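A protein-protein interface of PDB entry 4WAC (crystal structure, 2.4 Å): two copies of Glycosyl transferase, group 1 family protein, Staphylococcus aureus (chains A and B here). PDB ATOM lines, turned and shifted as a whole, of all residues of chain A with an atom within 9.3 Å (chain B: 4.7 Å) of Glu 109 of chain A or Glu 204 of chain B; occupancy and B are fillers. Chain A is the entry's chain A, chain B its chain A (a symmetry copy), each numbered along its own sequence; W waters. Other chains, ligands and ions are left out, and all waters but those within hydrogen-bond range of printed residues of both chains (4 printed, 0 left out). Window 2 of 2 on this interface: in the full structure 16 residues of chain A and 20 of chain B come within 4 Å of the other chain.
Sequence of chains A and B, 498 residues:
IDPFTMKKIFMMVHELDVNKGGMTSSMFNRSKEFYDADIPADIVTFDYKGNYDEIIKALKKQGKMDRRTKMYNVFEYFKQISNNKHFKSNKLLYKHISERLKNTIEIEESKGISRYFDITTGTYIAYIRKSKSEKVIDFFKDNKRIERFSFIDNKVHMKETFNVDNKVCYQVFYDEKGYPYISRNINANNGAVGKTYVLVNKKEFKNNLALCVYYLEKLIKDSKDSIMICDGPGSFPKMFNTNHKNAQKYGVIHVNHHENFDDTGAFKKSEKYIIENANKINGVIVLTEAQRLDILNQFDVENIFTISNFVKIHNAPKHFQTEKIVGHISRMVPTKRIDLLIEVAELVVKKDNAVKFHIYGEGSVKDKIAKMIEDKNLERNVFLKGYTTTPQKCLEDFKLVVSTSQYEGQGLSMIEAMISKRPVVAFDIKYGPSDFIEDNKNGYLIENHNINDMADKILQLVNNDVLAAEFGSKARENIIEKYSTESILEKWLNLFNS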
ATOM      1  N   GLU A 106      -7.779  25.395 -35.671  1.00  0.00           N
ATOM      2  CA  GLU A 106      -7.345  25.096 -34.336  1.00  0.00           C
ATOM      3  C   GLU A 106      -8.358  25.586 -33.343  1.00  0.00           C
ATOM      4  O   GLU A 106      -8.840  26.704 -33.468  1.00  0.00           O
ATOM      5  CB  GLU A 106      -6.008  25.772 -34.051  1.00  0.00           C
ATOM      6  CG  GLU A 106      -5.441  25.467 -32.707  1.00  0.00           C
ATOM      7  CD  GLU A 106      -4.275  26.369 -32.376  1.00  0.00           C
ATOM      8  OE1 GLU A 106      -4.027  27.316 -33.150  1.00  0.00           O
ATOM      9  OE2 GLU A 106      -3.573  26.092 -31.385  1.00  0.00           O
ATOM     10  N   ILE A 107      -8.662  24.773 -32.335  1.00  0.00           N
ATOM     11  CA  ILE A 107      -9.513  25.269 -31.251  1.00  0.00           C
ATOM     12  C   ILE A 107      -8.807  25.015 -29.918  1.00  0.00           C
ATOM     13  O   ILE A 107      -8.628  23.848 -29.489  1.00  0.00           O
ATOM     14  CB  ILE A 107     -10.899  24.606 -31.265  1.00  0.00           C
ATOM     15  CG1 ILE A 107     -11.575  24.866 -32.601  1.00  0.00           C
ATOM     16  CG2 ILE A 107     -11.763  25.144 -30.137  1.00  0.00           C
ATOM     17  CD1 ILE A 107     -12.977  24.414 -32.629  1.00  0.00           C
ATOM     18  N   GLU A 108      -8.362  26.101 -29.299  1.00  0.00           N
ATOM     19  CA  GLU A 108      -7.622  26.030 -28.053  1.00  0.00           C
ATOM     20  C   GLU A 108      -8.412  25.521 -26.865  1.00  0.00           C
ATOM     21  O   GLU A 108      -9.589  25.845 -26.701  1.00  0.00           O
ATOM     22  CB  GLU A 108      -7.067  27.401 -27.731  1.00  0.00           C
ATOM     23  CG  GLU A 108      -6.229  27.877 -28.871  1.00  0.00           C
ATOM     24  CD  GLU A 108      -5.496  29.129 -28.547  1.00  0.00           C
ATOM     25  OE1 GLU A 108      -5.640  29.612 -27.404  1.00  0.00           O
ATOM     26  OE2 GLU A 108      -4.762  29.615 -29.430  1.00  0.00           O
ATOM     27  N   GLU A 109      -7.765  24.702 -26.045  1.00  0.00           N
ATOM     28  CA  GLU A 109      -8.351  24.340 -24.768  1.00  0.00           C
ATOM     29  C   GLU A 109      -7.714  25.122 -23.623  1.00  0.00           C
ATOM     30  O   GLU A 109      -8.382  25.511 -22.686  1.00  0.00           O
ATOM     31  CB  GLU A 109      -8.206  22.859 -24.518  1.00  0.00           C
ATOM     32  CG  GLU A 109      -8.606  22.437 -23.104  1.00  0.00           C
ATOM     33  CD  GLU A 109      -8.463  20.934 -22.896  1.00  0.00           C
ATOM     34  OE1 GLU A 109      -7.789  20.538 -21.929  1.00  0.00           O
ATOM     35  OE2 GLU A 109      -9.038  20.153 -23.680  1.00  0.00           O
ATOM     36  N   SER A 110      -6.411  25.331 -23.730  1.00  0.00           N
ATOM     37  CA  SER A 110      -5.643  26.140 -22.796  1.00  0.00           C
ATOM     38  C   SER A 110      -4.312  26.338 -23.499  1.00  0.00           C
ATOM     39  O   SER A 110      -4.146  25.869 -24.628  1.00  0.00           O
ATOM     40  CB  SER A 110      -5.466  25.468 -21.442  1.00  0.00           C
ATOM     41  OG  SER A 110      -4.845  24.208 -21.576  1.00  0.00           O
ATOM     42  N   LYS A 111      -3.363  26.980 -22.842  1.00  0.00           N
ATOM     43  CA  LYS A 111      -2.221  27.574 -23.549  1.00  0.00           C
ATOM     44  C   LYS A 111      -1.341  26.582 -24.311  1.00  0.00           C
ATOM     45  O   LYS A 111      -0.790  26.917 -25.367  1.00  0.00           O
ATOM     46  CB  LYS A 111      -1.348  28.371 -22.574  1.00  0.00           C
ATOM     47  CG  LYS A 111       0.003  28.780 -23.156  1.00  0.00           C
ATOM     48  CD  LYS A 111       1.141  28.528 -22.192  1.00  0.00           C
ATOM     49  CE  LYS A 111       2.394  29.272 -22.621  1.00  0.00           C
ATOM     50  NZ  LYS A 111       3.206  29.661 -21.428  1.00  0.00           N
ATOM     51  N   GLY A 112      -1.211  25.369 -23.803  1.00  0.00           N
ATOM     52  CA  GLY A 112      -0.505  24.351 -24.573  1.00  0.00           C
ATOM     53  C   GLY A 112      -1.325  23.173 -25.080  1.00  0.00           C
ATOM     54  O   GLY A 112      -0.778  22.135 -25.431  1.00  0.00           O
ATOM     55  N   ILE A 113      -2.639  23.311 -25.126  1.00  0.00           N
ATOM     56  CA  ILE A 113      -3.484  22.205 -25.539  1.00  0.00           C
ATOM     57  C   ILE A 113      -4.515  22.697 -26.528  1.00  0.00           C
ATOM     58  O   ILE A 113      -5.364  23.533 -26.192  1.00  0.00           O
ATOM     59  CB  ILE A 113      -4.205  21.575 -24.350  1.00  0.00           C
ATOM     60  CG1 ILE A 113      -3.205  21.075 -23.318  1.00  0.00           C
ATOM     61  CG2 ILE A 113      -5.124  20.458 -24.805  1.00  0.00           C
ATOM     62  CD1 ILE A 113      -3.870  20.652 -22.043  1.00  0.00           C
ATOM     63  N   SER A 114      -4.444  22.168 -27.744  1.00  0.00           N
ATOM     64  CA  SER A 114      -5.396  22.521 -28.790  1.00  0.00           C
ATOM     65  C   SER A 114      -5.882  21.322 -29.556  1.00  0.00           C
ATOM     66  O   SER A 114      -5.200  20.277 -29.600  1.00  0.00           O
ATOM     67  CB  SER A 114      -4.769  23.511 -29.769  1.00  0.00           C
ATOM     68  OG  SER A 114      -4.533  24.733 -29.125  1.00  0.00           O
ATOM     69  N   ARG A 115      -7.038  21.495 -30.194  1.00  0.00           N
ATOM     70  CA  ARG A 115      -7.609  20.475 -31.090  1.00  0.00           C
ATOM     71  C   ARG A 115      -7.747  21.012 -32.496  1.00  0.00           C
ATOM     72  O   ARG A 115      -7.909  22.234 -32.705  1.00  0.00           O
ATOM     73  CB  ARG A 115      -8.961  20.005 -30.578  1.00  0.00           C
ATOM     74  CG  ARG A 115      -8.884  19.138 -29.332  1.00  0.00           C
ATOM     75  CD  ARG A 115     -10.284  18.830 -28.754  1.00  0.00           C
ATOM     76  NE  ARG A 115     -10.166  17.943 -27.606  1.00  0.00           N
ATOM     77  CZ  ARG A 115      -9.900  18.341 -26.364  1.00  0.00           C
ATOM     78  NH1 ARG A 115      -9.783  17.434 -25.403  1.00  0.00           N
ATOM     79  NH2 ARG A 115      -9.762  19.636 -26.073  1.00  0.00           N
ATOM     80  N   TYR A 116      -7.753  20.099 -33.460  1.00  0.00           N
ATOM     81  CA  TYR A 116      -7.736  20.466 -34.872  1.00  0.00           C
ATOM     82  C   TYR A 116      -8.853  19.762 -35.654  1.00  0.00           C
ATOM     83  O   TYR A 116      -9.020  18.540 -35.580  1.00  0.00           O
ATOM     84  CB  TYR A 116      -6.345  20.155 -35.462  1.00  0.00           C
ATOM     85  CG  TYR A 116      -5.239  20.990 -34.821  1.00  0.00           C
ATOM     86  CD1 TYR A 116      -4.660  20.629 -33.593  1.00  0.00           C
ATOM     87  CD2 TYR A 116      -4.793  22.156 -35.434  1.00  0.00           C
ATOM     88  CE1 TYR A 116      -3.635  21.437 -32.991  1.00  0.00           C
ATOM     89  CE2 TYR A 116      -3.804  22.957 -34.854  1.00  0.00           C
ATOM     90  CZ  TYR A 116      -3.215  22.593 -33.642  1.00  0.00           C
ATOM     91  OH  TYR A 116      -2.245  23.419 -33.109  1.00  0.00           O
ATOM     92  N   PHE A 117      -9.611  20.541 -36.419  1.00  0.00           N
ATOM     93  CA  PHE A 117     -10.794  20.052 -37.105  1.00  0.00           C
ATOM     94  C   PHE A 117     -10.700  20.369 -38.576  1.00  0.00           C
ATOM     95  O   PHE A 117     -10.326  21.479 -38.940  1.00  0.00           O
ATOM     96  CB  PHE A 117     -12.063  20.677 -36.511  1.00  0.00           C
ATOM     97  CG  PHE A 117     -12.297  20.334 -35.072  1.00  0.00           C
ATOM     98  CD1 PHE A 117     -11.663  21.051 -34.054  1.00  0.00           C
ATOM     99  CD2 PHE A 117     -13.154  19.274 -34.721  1.00  0.00           C
ATOM    100  CE1 PHE A 117     -11.869  20.715 -32.708  1.00  0.00           C
ATOM    101  CE2 PHE A 117     -13.378  18.943 -33.360  1.00  0.00           C
ATOM    102  CZ  PHE A 117     -12.729  19.668 -32.353  1.00  0.00           C
ATOM    103  N   TYR A 124     -13.031  15.596 -36.541  1.00  0.00           N
ATOM    104  CA  TYR A 124     -12.008  15.745 -35.497  1.00  0.00           C
ATOM    105  C   TYR A 124     -10.705  15.104 -35.966  1.00  0.00           C
ATOM    106  O   TYR A 124     -10.677  13.911 -36.221  1.00  0.00           O
ATOM    107  CB  TYR A 124     -12.473  15.092 -34.213  1.00  0.00           C
ATOM    108  CG  TYR A 124     -11.560  15.253 -33.009  1.00  0.00           C
ATOM    109  CD1 TYR A 124     -10.698  16.343 -32.890  1.00  0.00           C
ATOM    110  CD2 TYR A 124     -11.567  14.307 -31.975  1.00  0.00           C
ATOM    111  CE1 TYR A 124      -9.875  16.493 -31.796  1.00  0.00           C
ATOM    112  CE2 TYR A 124     -10.747  14.463 -30.855  1.00  0.00           C
ATOM    113  CZ  TYR A 124      -9.899  15.557 -30.791  1.00  0.00           C
ATOM    114  OH  TYR A 124      -9.091  15.758 -29.710  1.00  0.00           O
ATOM    115  N   TYR A 127      -5.375  16.090 -31.516  1.00  0.00           N
ATOM    116  CA  TYR A 127      -5.226  16.739 -30.231  1.00  0.00           C
ATOM    117  C   TYR A 127      -3.715  16.961 -30.004  1.00  0.00           C
ATOM    118  O   TYR A 127      -2.927  16.035 -30.145  1.00  0.00           O
ATOM    119  CB  TYR A 127      -5.861  15.878 -29.133  1.00  0.00           C
ATOM    120  CG  TYR A 127      -5.498  16.224 -27.695  1.00  0.00           C
ATOM    121  CD1 TYR A 127      -4.329  15.727 -27.109  1.00  0.00           C
ATOM    122  CD2 TYR A 127      -6.359  16.972 -26.898  1.00  0.00           C
ATOM    123  CE1 TYR A 127      -4.019  15.994 -25.766  1.00  0.00           C
ATOM    124  CE2 TYR A 127      -6.070  17.238 -25.575  1.00  0.00           C
ATOM    125  CZ  TYR A 127      -4.892  16.752 -25.012  1.00  0.00           C
ATOM    126  OH  TYR A 127      -4.590  17.030 -23.684  1.00  0.00           O
ATOM    127  N   ILE A 128      -3.322  18.185 -29.701  1.00  0.00           N
ATOM    128  CA  ILE A 128      -1.915  18.454 -29.468  1.00  0.00           C
ATOM    129  C   ILE A 128      -1.692  19.070 -28.103  1.00  0.00           C
ATOM    130  O   ILE A 128      -2.320  20.071 -27.740  1.00  0.00           O
ATOM    131  CB  ILE A 128      -1.334  19.362 -30.539  1.00  0.00           C
ATOM    132  CG1 ILE A 128      -1.546  18.694 -31.905  1.00  0.00           C
ATOM    133  CG2 ILE A 128       0.182  19.562 -30.282  1.00  0.00           C
ATOM    134  CD1 ILE A 128      -0.819  19.389 -33.069  1.00  0.00           C
ATOM    135  N   ARG A 129      -0.821  18.431 -27.336  1.00  0.00           N
ATOM    136  CA  ARG A 129      -0.442  18.939 -26.032  1.00  0.00           C
ATOM    137  C   ARG A 129       1.060  19.141 -26.001  1.00  0.00           C
ATOM    138  O   ARG A 129       1.835  18.254 -26.401  1.00  0.00           O
ATOM    139  CB  ARG A 129      -0.876  18.002 -24.904  1.00  0.00           C
ATOM    140  CG  ARG A 129      -0.489  18.579 -23.521  1.00  0.00           C
ATOM    141  CD  ARG A 129      -1.136  17.837 -22.335  1.00  0.00           C
ATOM    142  NE  ARG A 129      -0.656  16.453 -22.255  1.00  0.00           N
ATOM    143  CZ  ARG A 129      -1.408  15.369 -22.464  1.00  0.00           C
ATOM    144  NH1 ARG A 129      -2.701  15.494 -22.783  1.00  0.00           N
ATOM    145  NH2 ARG A 129      -0.863  14.151 -22.362  1.00  0.00           N
ATOM    146  N   LYS B 195     -18.726  17.544 -25.266  1.00  0.00           N
ATOM    147  CA  LYS B 195     -17.917  18.617 -25.836  1.00  0.00           C
ATOM    148  C   LYS B 195     -18.566  19.104 -27.131  1.00  0.00           C
ATOM    149  O   LYS B 195     -18.909  18.292 -27.977  1.00  0.00           O
ATOM    150  CB  LYS B 195     -16.470  18.151 -26.112  1.00  0.00           C
ATOM    151  CG  LYS B 195     -15.607  17.874 -24.854  1.00  0.00           C
ATOM    152  CD  LYS B 195     -15.387  19.143 -24.036  1.00  0.00           C
ATOM    153  CE  LYS B 195     -14.686  20.251 -24.824  1.00  0.00           C
ATOM    154  NZ  LYS B 195     -13.311  19.761 -25.266  1.00  0.00           N
ATOM    155  N   THR B 196     -18.781  20.419 -27.229  1.00  0.00           N
ATOM    156  CA  THR B 196     -19.341  21.057 -28.409  1.00  0.00           C
ATOM    157  C   THR B 196     -18.377  22.073 -28.987  1.00  0.00           C
ATOM    158  O   THR B 196     -17.920  22.988 -28.271  1.00  0.00           O
ATOM    159  CB  THR B 196     -20.676  21.769 -28.083  1.00  0.00           C
ATOM    160  OG1 THR B 196     -21.597  20.807 -27.573  1.00  0.00           O
ATOM    161  CG2 THR B 196     -21.289  22.380 -29.311  1.00  0.00           C
ATOM    162  N   TYR B 197     -18.078  21.941 -30.274  1.00  0.00           N
ATOM    163  CA  TYR B 197     -17.083  22.817 -30.890  1.00  0.00           C
ATOM    164  C   TYR B 197     -17.759  23.776 -31.851  1.00  0.00           C
ATOM    165  O   TYR B 197     -18.365  23.355 -32.846  1.00  0.00           O
ATOM    166  CB  TYR B 197     -15.991  21.973 -31.591  1.00  0.00           C
ATOM    167  CG  TYR B 197     -15.288  21.060 -30.609  1.00  0.00           C
ATOM    168  CD1 TYR B 197     -14.298  21.569 -29.745  1.00  0.00           C
ATOM    169  CD2 TYR B 197     -15.616  19.701 -30.528  1.00  0.00           C
ATOM    170  CE1 TYR B 197     -13.654  20.736 -28.816  1.00  0.00           C
ATOM    171  CE2 TYR B 197     -14.982  18.864 -29.638  1.00  0.00           C
ATOM    172  CZ  TYR B 197     -14.010  19.383 -28.770  1.00  0.00           C
ATOM    173  OH  TYR B 197     -13.419  18.559 -27.860  1.00  0.00           O
ATOM    174  N   LYS B 202     -14.192  29.330 -33.683  1.00  0.00           N
ATOM    175  CA  LYS B 202     -13.015  28.710 -33.079  1.00  0.00           C
ATOM    176  C   LYS B 202     -13.121  28.602 -31.558  1.00  0.00           C
ATOM    177  O   LYS B 202     -12.194  28.952 -30.850  1.00  0.00           O
ATOM    178  CB  LYS B 202     -11.739  29.484 -33.469  1.00  0.00           C
ATOM    179  CG  LYS B 202     -11.279  29.073 -34.856  1.00  0.00           C
ATOM    180  CD  LYS B 202     -10.631  30.199 -35.619  1.00  0.00           C
ATOM    181  CE  LYS B 202      -9.130  30.014 -35.774  1.00  0.00           C
ATOM    182  NZ  LYS B 202      -8.331  30.183 -34.496  1.00  0.00           N
ATOM    183  N   LYS B 203     -14.260  28.143 -31.053  1.00  0.00           N
ATOM    184  CA  LYS B 203     -14.461  28.140 -29.595  1.00  0.00           C
ATOM    185  C   LYS B 203     -15.005  26.787 -29.150  1.00  0.00           C
ATOM    186  O   LYS B 203     -15.793  26.185 -29.873  1.00  0.00           O
ATOM    187  CB  LYS B 203     -15.433  29.265 -29.165  1.00  0.00           C
ATOM    188  CG  LYS B 203     -15.301  29.627 -27.704  1.00  0.00           C
ATOM    189  CD  LYS B 203     -16.259  30.723 -27.265  1.00  0.00           C
ATOM    190  CE  LYS B 203     -15.921  31.220 -25.840  1.00  0.00           C
ATOM    191  NZ  LYS B 203     -15.641  30.138 -24.853  1.00  0.00           N
ATOM    192  N   GLU B 204     -14.613  26.323 -27.963  1.00  0.00           N
ATOM    193  CA  GLU B 204     -15.122  25.041 -27.448  1.00  0.00           C
ATOM    194  C   GLU B 204     -16.001  25.256 -26.224  1.00  0.00           C
ATOM    195  O   GLU B 204     -15.904  26.272 -25.551  1.00  0.00           O
ATOM    196  CB  GLU B 204     -13.972  24.061 -27.114  1.00  0.00           C
ATOM    197  CG  GLU B 204     -13.026  24.525 -25.963  1.00  0.00           C
ATOM    198  CD  GLU B 204     -12.207  23.367 -25.394  1.00  0.00           C
ATOM    199  OE1 GLU B 204     -11.758  23.427 -24.229  1.00  0.00           O
ATOM    200  OE2 GLU B 204     -12.045  22.364 -26.108  1.00  0.00           O
ATOM    201  N   PHE B 205     -16.900  24.312 -25.972  1.00  0.00           N
ATOM    202  CA  PHE B 205     -17.749  24.374 -24.792  1.00  0.00           C
ATOM    203  C   PHE B 205     -17.765  23.010 -24.169  1.00  0.00           C
ATOM    204  O   PHE B 205     -17.645  21.976 -24.883  1.00  0.00           O
ATOM    205  CB  PHE B 205     -19.169  24.829 -25.173  1.00  0.00           C
ATOM    206  CG  PHE B 205     -19.222  26.263 -25.653  1.00  0.00           C
ATOM    207  CD1 PHE B 205     -19.014  26.569 -26.993  1.00  0.00           C
ATOM    208  CD2 PHE B 205     -19.417  27.309 -24.745  1.00  0.00           C
ATOM    209  CE1 PHE B 205     -19.029  27.913 -27.430  1.00  0.00           C
ATOM    210  CE2 PHE B 205     -19.426  28.642 -25.167  1.00  0.00           C
ATOM    211  CZ  PHE B 205     -19.239  28.951 -26.509  1.00  0.00           C
ATOM    212  N   LYS B 206     -17.972  22.974 -22.866  1.00  0.00           N
ATOM    213  CA  LYS B 206     -18.041  21.693 -22.153  1.00  0.00           C
ATOM    214  C   LYS B 206     -19.165  20.821 -22.691  1.00  0.00           C
ATOM    215  O   LYS B 206     -18.996  19.615 -22.848  1.00  0.00           O
ATOM    216  CB  LYS B 206     -18.243  21.914 -20.644  1.00  0.00           C
ATOM    217  CG  LYS B 206     -18.227  20.616 -19.814  1.00  0.00           C
ATOM    218  CD  LYS B 206     -18.506  20.913 -18.311  1.00  0.00           C
ATOM    219  CE  LYS B 206     -18.431  19.654 -17.436  1.00  0.00           C
ATOM    220  NZ  LYS B 206     -18.879  19.895 -16.026  1.00  0.00           N
HETATM  221  O   HOH W   1     -11.214  25.747 -23.040  1.00  0.00           O
HETATM  222  O   HOH W   2      -9.307  28.713 -30.442  1.00  0.00           O
HETATM  223  O   HOH W   3     -10.019  22.033 -27.691  1.00  0.00           O
HETATM  224  O   HOH W   4     -11.735  27.456 -27.087  1.00  0.00           O
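The guanidinium group (NE) of Arg 115 of chain A lies close to the side-chain hydroxyl (OH) of Tyr 197 of chain B (3.3 Å).
The side-chain carboxylate of Glu 204 of chain B is in salt-bridge range of the guanidinium group of Arg 115 of chain A.
The backbone NH of Ile 107 of chain A sits at hydrogen-bond distance from the backbone carbonyl oxygen of Arg 115 of chain A (2.7 Å).
NZ of Lys 195 of chain B is in hydrogen-bond range of OH of Tyr 197 of chain B, 2.9 Å away.
OE2 of Glu 106 of chain A is in hydrogen-bond range of OG of Ser 114 of chain A (2.8 Å).
NH2 of Arg 115 of chain A is in salt-bridge range of OE2 of Glu 109 of chain A (2.6 Å).
NZ of Lys 195 of chain B lies within salt-bridge range of OE2 of Glu 204 of chain B (3.0 Å).
The backbone NH (N) of Lys 195 of chain B sits at hydrogen-bond distance from the backbone carbonyl oxygen (O) of Lys 206 of chain B.
Among the printed residues, pairs that only touch across the chains: Glu 106 of chain A with Lys 202 of chain B (3.7 Å), Ile 107 of chain A with Lys 202 of chain B (3.9 Å), Ile 107 of chain A with Lys 203 of chain B (3.8 Å), Ile 107 of chain A with Glu 204 of chain B (3.8 Å), Glu 108 of chain A with Glu 204 of chain B (3.8 Å), Glu 109 of chain A with Glu 204 of chain B (3.5 Å), Arg 115 of chain A with Lys 195 of chain B (3.6 Å) and Phe 117 of chain A with Tyr 197 of chain B (3.4 Å).
Of the printed residues of chain B, Glu 109 of chain A touches Glu 204.
Of the printed residues of chain A, Glu 204 of chain B touches Ile 107 (3.8 Å), Glu 108 (3.8 Å), Glu 109 (3.5 Å) and Arg 115 (3.6 Å).
Lys 203 of chain B touches one residue of chain A.
No residue of chain A comes within 4 Å of Phe 205 of chain B.
Printed residues of chain B within 4 Å of Arg 115 of chain A: Lys 195 (3.6 Å), Tyr 197 (3.3 Å) and Glu 204 (3.6 Å).
Of the printed residues of chain A, Tyr 197 of chain B touches Arg 115 and Phe 117.
Of the printed residues of chain A, Lys 195 of chain B touches Arg 115.
Lys 111 of chain A touches none of the printed residues of chain B.
Gly 112 of chain A touches none of the printed residues of chain B.
The nearest residue of chain B that does not touch Glu 109 of chain A is Lys 195 of chain B (4.6 Å).
The nearest residue of chain A that does not touch Glu 204 of chain B is Ser 110 of chain A (5.7 Å).
Printed residues of chain A that touch a printed residue of chain B: Glu 106, Ile 107, Glu 108, Glu 109, Arg 115 and Phe 117.
Of the 8 printed residues of chain B, 5 touch a printed residue of chain A.
Hydrophobic or aromatic side chains of chain B that line the printed part of chain A: Tyr 197.
Among the printed residues, Asp or Glu carboxylates within 4 Å of a Lys or Arg side-chain nitrogen of the other chain: Arg 115 of chain A with Glu 204 of chain B.
No position is printed for both chains.
Of the 10 pairs that touch across the chains among the printed residues, none has its exchanged pair printed and touching as well.
Water W3 lies within hydrogen-bond range of the side-chain carboxylate of Glu 204 of chain B, the guanidinium group of Arg 115 of chain A and the backbone carbonyl oxygen of Ile 107 of chain A.
Water W1 bridges OE1 of Glu 204 of chain B and O of Glu 109 of chain A.
Water W4 bridges O of Glu 108 of chain A and N of Glu 204 of chain B.
Water W2 bridges O of Lys 202 of chain B and N of Glu 108 of chain A.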
